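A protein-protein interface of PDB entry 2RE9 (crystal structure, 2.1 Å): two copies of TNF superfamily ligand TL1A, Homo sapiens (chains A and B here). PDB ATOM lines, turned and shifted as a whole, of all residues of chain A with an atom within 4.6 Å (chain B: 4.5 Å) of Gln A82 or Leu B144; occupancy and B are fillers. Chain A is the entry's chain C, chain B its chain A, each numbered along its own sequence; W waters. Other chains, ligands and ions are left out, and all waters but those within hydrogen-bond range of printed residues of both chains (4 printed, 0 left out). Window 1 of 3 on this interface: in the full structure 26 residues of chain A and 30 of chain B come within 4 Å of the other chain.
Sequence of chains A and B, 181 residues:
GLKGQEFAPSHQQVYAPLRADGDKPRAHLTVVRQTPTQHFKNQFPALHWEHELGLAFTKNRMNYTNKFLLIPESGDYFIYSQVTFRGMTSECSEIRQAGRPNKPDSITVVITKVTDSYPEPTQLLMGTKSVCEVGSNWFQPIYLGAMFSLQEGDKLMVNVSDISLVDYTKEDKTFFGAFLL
The side-chain amide nitrogen (NE2) of Gln A82 lies within hydrogen-bond range of the backbone carbonyl oxygen (O) of Met B126 (3.0 Å).
The backbone carbonyl oxygen (O) of Asp A172 is in hydrogen-bond range of the backbone NH (N) of Met B126.
The side-chain hydroxyl of Tyr A143 sits at hydrogen-bond distance from the backbone carbonyl oxygen of Gly B145 (2.9 Å).
Tyr A143 touches its own counterpart, Tyr B143.
Positions printed for both chains: 81, 142 and 143.
Of the 10 pairs that touch across the chains among the printed residues, 1 has its exchanged pair printed and touching as well.
Printed residues of chain B within 4 Å of Gln A82: Met B126 (3.0 Å), Tyr B143 (3.99 Å) and Leu B144 (3.2 Å).
Of chain A, only Gln A82 (3.2 Å) comes within 4 Å of Leu B144.
Of the printed residues of chain B, Lys A173 touches Met B126.
Of the printed residues of chain B, Phe A175 touches Leu B125 (3.5 Å) and Gly B145 (3.7 Å).
Thr A174 touches none of the printed residues of chain B.
Ser B81 touches none of the printed residues of chain A.
The nearest residue of chain A that does not touch Leu B144 is Tyr A143 (4.5 Å).
Printed residues of chain B that touch a printed residue of chain A: Leu B125, Met B126, Tyr B143, Leu B144 and Gly B145.
Hydrophobic or aromatic side chains of chain B within 4 Å of the printed part of chain A: Leu B125, Met B126, Tyr B143 and Leu B144.
Along chain B the printed residues that touch a printed residue of chain A span positions 125 to 145.
Hydrophobic or aromatic side chains of chain A within 4 Å of the printed part of chain B: Tyr A143 and Phe A175.
Among the printed residues, no Asp or Glu carboxylate lies within 4 Å of a Lys or Arg side-chain nitrogen of the other chain.
The backbone NH of Ser B81 lies within hydrogen-bond range of the backbone carbonyl oxygen of Leu B144, 2.8 Å away.
O of Phe A175 lies within hydrogen-bond range of OG of Ser A81 (2.9 Å).
The backbone carbonyl oxygen (O) of Lys A173 lies within hydrogen-bond range of the side-chain amide nitrogen (NE2) of Gln A82 (2.9 Å).
The backbone carbonyl oxygen (O) of Gln A82 lies within hydrogen-bond range of the backbone NH (N) of Phe A175 (3.0 Å).
OG1 of Thr A84 sits at hydrogen-bond distance from O of Lys A173 (2.7 Å).
Water W3 bridges the backbone carbonyl oxygen of Tyr B143 (2.5 Å) and the side-chain amide oxygen of Gln A82 (2.6 Å).
Water W4 bridges the side-chain hydroxyl (OG1) of Thr A84 and the backbone carbonyl oxygen (O) of Met B126.
Water W2 bridges the side-chain carboxylate (OD1) of Asp A172 (2.9 Å) and the side-chain sulfur (SD) of Met B126 (3.7 Å).
Water W1 bridges OH of Tyr B143 and OH of Tyr A143.
Among the printed residues, pairs that only touch across the chains: Gln A82 with Leu B144, Tyr A143 with Tyr B143, Phe A175 with Leu B125, Asp A172 with Leu B125, Phe A175 with Gly B145, Lys A173 with Met B126 and Gln A82 with Tyr B143.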
ATOM      1  N   SER A  81       6.183   9.177   9.437  1.00  0.00           N
ATOM      2  CA  SER A  81       6.091   7.746   9.334  1.00  0.00           C
ATOM      3  C   SER A  81       4.801   7.241   9.933  1.00  0.00           C
ATOM      4  O   SER A  81       4.258   7.843  10.859  1.00  0.00           O
ATOM      5  CB  SER A  81       7.272   7.098  10.054  1.00  0.00           C
ATOM      6  OG  SER A  81       7.105   5.695  10.160  1.00  0.00           O
ATOM      7  N   GLN A  82       4.284   6.161   9.364  1.00  0.00           N
ATOM      8  CA  GLN A  82       3.103   5.521   9.915  1.00  0.00           C
ATOM      9  C   GLN A  82       3.430   4.047   9.960  1.00  0.00           C
ATOM     10  O   GLN A  82       4.064   3.509   9.050  1.00  0.00           O
ATOM     11  CB  GLN A  82       1.842   5.730   9.070  1.00  0.00           C
ATOM     12  CG  GLN A  82       0.699   4.840   9.560  1.00  0.00           C
ATOM     13  CD  GLN A  82      -0.641   5.109   8.893  1.00  0.00           C
ATOM     14  OE1 GLN A  82      -1.338   6.070   9.233  1.00  0.00           O
ATOM     15  NE2 GLN A  82      -1.015   4.249   7.942  1.00  0.00           N
ATOM     16  N   VAL A  83       3.031   3.401  11.039  1.00  0.00           N
ATOM     17  CA  VAL A  83       3.260   1.983  11.184  1.00  0.00           C
ATOM     18  C   VAL A  83       1.951   1.394  11.639  1.00  0.00           C
ATOM     19  O   VAL A  83       1.431   1.752  12.693  1.00  0.00           O
ATOM     20  CB  VAL A  83       4.345   1.673  12.232  1.00  0.00           C
ATOM     21  CG1 VAL A  83       4.469   0.168  12.404  1.00  0.00           C
ATOM     22  CG2 VAL A  83       5.676   2.257  11.791  1.00  0.00           C
ATOM     23  N   THR A  84       1.398   0.510  10.828  1.00  0.00           N
ATOM     24  CA  THR A  84       0.143  -0.113  11.191  1.00  0.00           C
ATOM     25  C   THR A  84       0.477  -1.396  11.924  1.00  0.00           C
ATOM     26  O   THR A  84       1.288  -2.186  11.451  1.00  0.00           O
ATOM     27  CB  THR A  84      -0.699  -0.413   9.938  1.00  0.00           C
ATOM     28  OG1 THR A  84      -0.997   0.821   9.273  1.00  0.00           O
ATOM     29  CG2 THR A  84      -2.009  -1.120  10.318  1.00  0.00           C
ATOM     30  N   PRO A 141      -3.078   2.099  13.325  1.00  0.00           N
ATOM     31  CA  PRO A 141      -1.861   2.779  12.910  1.00  0.00           C
ATOM     32  C   PRO A 141      -1.415   3.810  13.926  1.00  0.00           C
ATOM     33  O   PRO A 141      -2.198   4.277  14.749  1.00  0.00           O
ATOM     34  CB  PRO A 141      -2.279   3.424  11.601  1.00  0.00           C
ATOM     35  CG  PRO A 141      -3.667   3.896  11.929  1.00  0.00           C
ATOM     36  CD  PRO A 141      -4.266   2.736  12.724  1.00  0.00           C
ATOM     37  N   ILE A 142      -0.135   4.136  13.865  1.00  0.00           N
ATOM     38  CA  ILE A 142       0.451   5.158  14.705  1.00  0.00           C
ATOM     39  C   ILE A 142       1.131   6.049  13.676  1.00  0.00           C
ATOM     40  O   ILE A 142       1.989   5.592  12.935  1.00  0.00           O
ATOM     41  CB  ILE A 142       1.492   4.570  15.678  1.00  0.00           C
ATOM     42  CG1 ILE A 142       0.772   3.795  16.791  1.00  0.00           C
ATOM     43  CG2 ILE A 142       2.366   5.687  16.250  1.00  0.00           C
ATOM     44  CD1 ILE A 142       1.703   3.157  17.800  1.00  0.00           C
ATOM     45  N   TYR A 143       0.710   7.305  13.600  1.00  0.00           N
ATOM     46  CA  TYR A 143       1.292   8.242  12.651  1.00  0.00           C
ATOM     47  C   TYR A 143       2.096   9.296  13.411  1.00  0.00           C
ATOM     48  O   TYR A 143       1.673   9.755  14.469  1.00  0.00           O
ATOM     49  CB  TYR A 143       0.194   8.935  11.833  1.00  0.00           C
ATOM     50  CG  TYR A 143       0.754   9.905  10.820  1.00  0.00           C
ATOM     51  CD1 TYR A 143       1.118   9.480   9.545  1.00  0.00           C
ATOM     52  CD2 TYR A 143       1.005  11.234  11.168  1.00  0.00           C
ATOM     53  CE1 TYR A 143       1.726  10.355   8.640  1.00  0.00           C
ATOM     54  CE2 TYR A 143       1.609  12.111  10.277  1.00  0.00           C
ATOM     55  CZ  TYR A 143       1.965  11.665   9.013  1.00  0.00           C
ATOM     56  OH  TYR A 143       2.528  12.544   8.119  1.00  0.00           O
ATOM     57  N   ASP A 172       0.810   1.241   1.430  1.00  0.00           N
ATOM     58  CA  ASP A 172       0.035   2.391   1.872  1.00  0.00           C
ATOM     59  C   ASP A 172      -0.312   2.390   3.360  1.00  0.00           C
ATOM     60  O   ASP A 172      -0.864   3.364   3.862  1.00  0.00           O
ATOM     61  CB  ASP A 172      -1.252   2.525   1.042  1.00  0.00           C
ATOM     62  CG  ASP A 172      -2.169   1.328   1.183  1.00  0.00           C
ATOM     63  OD1 ASP A 172      -3.340   1.420   0.765  1.00  0.00           O
ATOM     64  OD2 ASP A 172      -1.723   0.289   1.708  1.00  0.00           O
ATOM     65  N   LYS A 173       0.012   1.309   4.067  1.00  0.00           N
ATOM     66  CA  LYS A 173      -0.296   1.237   5.492  1.00  0.00           C
ATOM     67  C   LYS A 173       0.902   1.479   6.408  1.00  0.00           C
ATOM     68  O   LYS A 173       0.737   1.910   7.550  1.00  0.00           O
ATOM     69  CB  LYS A 173      -0.946  -0.109   5.835  1.00  0.00           C
ATOM     70  CG  LYS A 173      -2.407  -0.186   5.416  1.00  0.00           C
ATOM     71  CD  LYS A 173      -3.139  -1.373   6.025  1.00  0.00           C
ATOM     72  CE  LYS A 173      -2.698  -2.681   5.406  1.00  0.00           C
ATOM     73  NZ  LYS A 173      -3.587  -3.800   5.836  1.00  0.00           N
ATOM     74  N   THR A 174       2.099   1.197   5.908  1.00  0.00           N
ATOM     75  CA  THR A 174       3.317   1.387   6.683  1.00  0.00           C
ATOM     76  C   THR A 174       4.356   2.037   5.791  1.00  0.00           C
ATOM     77  O   THR A 174       4.770   1.463   4.783  1.00  0.00           O
ATOM     78  CB  THR A 174       3.840   0.051   7.210  1.00  0.00           C
ATOM     79  OG1 THR A 174       2.866  -0.506   8.094  1.00  0.00           O
ATOM     80  CG2 THR A 174       5.151   0.239   7.973  1.00  0.00           C
ATOM     81  N   PHE A 175       4.776   3.238   6.167  1.00  0.00           N
ATOM     82  CA  PHE A 175       5.732   3.986   5.372  1.00  0.00           C
ATOM     83  C   PHE A 175       6.564   4.918   6.236  1.00  0.00           C
ATOM     84  O   PHE A 175       6.311   5.072   7.433  1.00  0.00           O
ATOM     85  CB  PHE A 175       4.996   4.794   4.297  1.00  0.00           C
ATOM     86  CG  PHE A 175       3.807   5.554   4.823  1.00  0.00           C
ATOM     87  CD1 PHE A 175       2.542   4.975   4.829  1.00  0.00           C
ATOM     88  CD2 PHE A 175       3.958   6.839   5.339  1.00  0.00           C
ATOM     89  CE1 PHE A 175       1.435   5.666   5.345  1.00  0.00           C
ATOM     90  CE2 PHE A 175       2.863   7.539   5.856  1.00  0.00           C
ATOM     91  CZ  PHE A 175       1.600   6.948   5.857  1.00  0.00           C
ATOM     92  N   ILE B  79       0.448  15.351   0.809  1.00  0.00           N
ATOM     93  CA  ILE B  79      -0.995  15.309   0.888  1.00  0.00           C
ATOM     94  C   ILE B  79      -1.355  14.812   2.274  1.00  0.00           C
ATOM     95  O   ILE B  79      -0.624  14.016   2.858  1.00  0.00           O
ATOM     96  CB  ILE B  79      -1.572  14.372  -0.194  1.00  0.00           C
ATOM     97  CG1 ILE B  79      -1.342  12.914   0.183  1.00  0.00           C
ATOM     98  CG2 ILE B  79      -0.867  14.638  -1.525  1.00  0.00           C
ATOM     99  CD1 ILE B  79      -1.790  11.936  -0.896  1.00  0.00           C
ATOM    100  N   TYR B  80      -2.480  15.273   2.801  1.00  0.00           N
ATOM    101  CA  TYR B  80      -2.871  14.865   4.139  1.00  0.00           C
ATOM    102  C   TYR B  80      -4.369  14.923   4.319  1.00  0.00           C
ATOM    103  O   TYR B  80      -5.073  15.640   3.611  1.00  0.00           O
ATOM    104  CB  TYR B  80      -2.213  15.790   5.161  1.00  0.00           C
ATOM    105  CG  TYR B  80      -2.701  17.217   5.036  1.00  0.00           C
ATOM    106  CD1 TYR B  80      -3.890  17.618   5.642  1.00  0.00           C
ATOM    107  CD2 TYR B  80      -1.998  18.156   4.272  1.00  0.00           C
ATOM    108  CE1 TYR B  80      -4.373  18.915   5.493  1.00  0.00           C
ATOM    109  CE2 TYR B  80      -2.473  19.459   4.115  1.00  0.00           C
ATOM    110  CZ  TYR B  80      -3.663  19.831   4.730  1.00  0.00           C
ATOM    111  OH  TYR B  80      -4.160  21.103   4.574  1.00  0.00           O
ATOM    112  N   SER B  81      -4.854  14.168   5.288  1.00  0.00           N
ATOM    113  CA  SER B  81      -6.269  14.166   5.575  1.00  0.00           C
ATOM    114  C   SER B  81      -6.547  13.597   6.946  1.00  0.00           C
ATOM    115  O   SER B  81      -5.834  12.725   7.429  1.00  0.00           O
ATOM    116  CB  SER B  81      -7.023  13.320   4.548  1.00  0.00           C
ATOM    117  OG  SER B  81      -8.398  13.224   4.887  1.00  0.00           O
ATOM    118  N   VAL B 109      -9.785   4.970   6.217  1.00  0.00           N
ATOM    119  CA  VAL B 109      -9.673   6.163   5.399  1.00  0.00           C
ATOM    120  C   VAL B 109      -8.594   5.803   4.391  1.00  0.00           C
ATOM    121  O   VAL B 109      -7.568   5.232   4.756  1.00  0.00           O
ATOM    122  CB  VAL B 109      -9.183   7.407   6.175  1.00  0.00           C
ATOM    123  CG1 VAL B 109      -9.030   8.575   5.200  1.00  0.00           C
ATOM    124  CG2 VAL B 109     -10.162   7.776   7.257  1.00  0.00           C
ATOM    125  N   LEU B 125      -2.376   6.172   0.563  1.00  0.00           N
ATOM    126  CA  LEU B 125      -2.321   6.039   2.017  1.00  0.00           C
ATOM    127  C   LEU B 125      -3.562   5.379   2.554  1.00  0.00           C
ATOM    128  O   LEU B 125      -4.660   5.610   2.052  1.00  0.00           O
ATOM    129  CB  LEU B 125      -2.245   7.402   2.713  1.00  0.00           C
ATOM    130  CG  LEU B 125      -1.060   8.335   2.577  1.00  0.00           C
ATOM    131  CD1 LEU B 125       0.236   7.553   2.682  1.00  0.00           C
ATOM    132  CD2 LEU B 125      -1.172   9.045   1.271  1.00  0.00           C
ATOM    133  N   MET B 126      -3.393   4.589   3.601  1.00  0.00           N
ATOM    134  CA  MET B 126      -4.533   3.955   4.228  1.00  0.00           C
ATOM    135  C   MET B 126      -4.366   3.888   5.726  1.00  0.00           C
ATOM    136  O   MET B 126      -3.336   3.458   6.229  1.00  0.00           O
ATOM    137  CB  MET B 126      -4.762   2.537   3.702  1.00  0.00           C
ATOM    138  CG  MET B 126      -5.943   1.858   4.389  1.00  0.00           C
ATOM    139  SD  MET B 126      -6.265   0.170   3.827  1.00  0.00           S
ATOM    140  CE  MET B 126      -7.159   0.481   2.344  1.00  0.00           C
ATOM    141  N   GLY B 127      -5.397   4.325   6.428  1.00  0.00           N
ATOM    142  CA  GLY B 127      -5.396   4.277   7.870  1.00  0.00           C
ATOM    143  C   GLY B 127      -6.626   3.478   8.229  1.00  0.00           C
ATOM    144  O   GLY B 127      -7.739   3.874   7.889  1.00  0.00           O
ATOM    145  N   ILE B 142      -8.762   9.579  12.338  1.00  0.00           N
ATOM    146  CA  ILE B 142      -7.711   8.838  11.674  1.00  0.00           C
ATOM    147  C   ILE B 142      -7.024   9.915  10.846  1.00  0.00           C
ATOM    148  O   ILE B 142      -7.671  10.582  10.033  1.00  0.00           O
ATOM    149  CB  ILE B 142      -8.270   7.740  10.752  1.00  0.00           C
ATOM    150  CG1 ILE B 142      -8.835   6.595  11.599  1.00  0.00           C
ATOM    151  CG2 ILE B 142      -7.174   7.245   9.822  1.00  0.00           C
ATOM    152  CD1 ILE B 142      -9.459   5.475  10.804  1.00  0.00           C
ATOM    153  N   TYR B 143      -5.731  10.114  11.078  1.00  0.00           N
ATOM    154  CA  TYR B 143      -4.977  11.125  10.356  1.00  0.00           C
ATOM    155  C   TYR B 143      -3.933  10.464   9.466  1.00  0.00           C
ATOM    156  O   TYR B 143      -3.288   9.497   9.870  1.00  0.00           O
ATOM    157  CB  TYR B 143      -4.282  12.084  11.333  1.00  0.00           C
ATOM    158  CG  TYR B 143      -3.444  13.128  10.640  1.00  0.00           C
ATOM    159  CD1 TYR B 143      -4.002  14.338  10.224  1.00  0.00           C
ATOM    160  CD2 TYR B 143      -2.113  12.874  10.319  1.00  0.00           C
ATOM    161  CE1 TYR B 143      -3.254  15.265   9.500  1.00  0.00           C
ATOM    162  CE2 TYR B 143      -1.358  13.790   9.599  1.00  0.00           C
ATOM    163  CZ  TYR B 143      -1.932  14.980   9.191  1.00  0.00           C
ATOM    164  OH  TYR B 143      -1.179  15.879   8.472  1.00  0.00           O
ATOM    165  N   LEU B 144      -3.769  10.997   8.258  1.00  0.00           N
ATOM    166  CA  LEU B 144      -2.806  10.466   7.290  1.00  0.00           C
ATOM    167  C   LEU B 144      -2.099  11.595   6.551  1.00  0.00           C
ATOM    168  O   LEU B 144      -2.718  12.596   6.209  1.00  0.00           O
ATOM    169  CB  LEU B 144      -3.519   9.606   6.240  1.00  0.00           C
ATOM    170  CG  LEU B 144      -4.144   8.270   6.613  1.00  0.00           C
ATOM    171  CD1 LEU B 144      -5.177   7.898   5.547  1.00  0.00           C
ATOM    172  CD2 LEU B 144      -3.056   7.199   6.724  1.00  0.00           C
ATOM    173  N   GLY B 145      -0.812  11.419   6.287  1.00  0.00           N
ATOM    174  CA  GLY B 145      -0.076  12.433   5.561  1.00  0.00           C
ATOM    175  C   GLY B 145       1.208  11.859   5.004  1.00  0.00           C
ATOM    176  O   GLY B 145       1.875  11.079   5.677  1.00  0.00           O
HETATM  177  O   HOH W   1       1.605  15.259   9.105  1.00  0.00           O
HETATM  178  O   HOH W   2      -4.334  -1.258   1.065  1.00  0.00           O
HETATM  179  O   HOH W   3      -3.479   7.023  10.457  1.00  0.00           O
HETATM  180  O   HOH W   4      -3.604   1.570   8.418  1.00  0.00           O
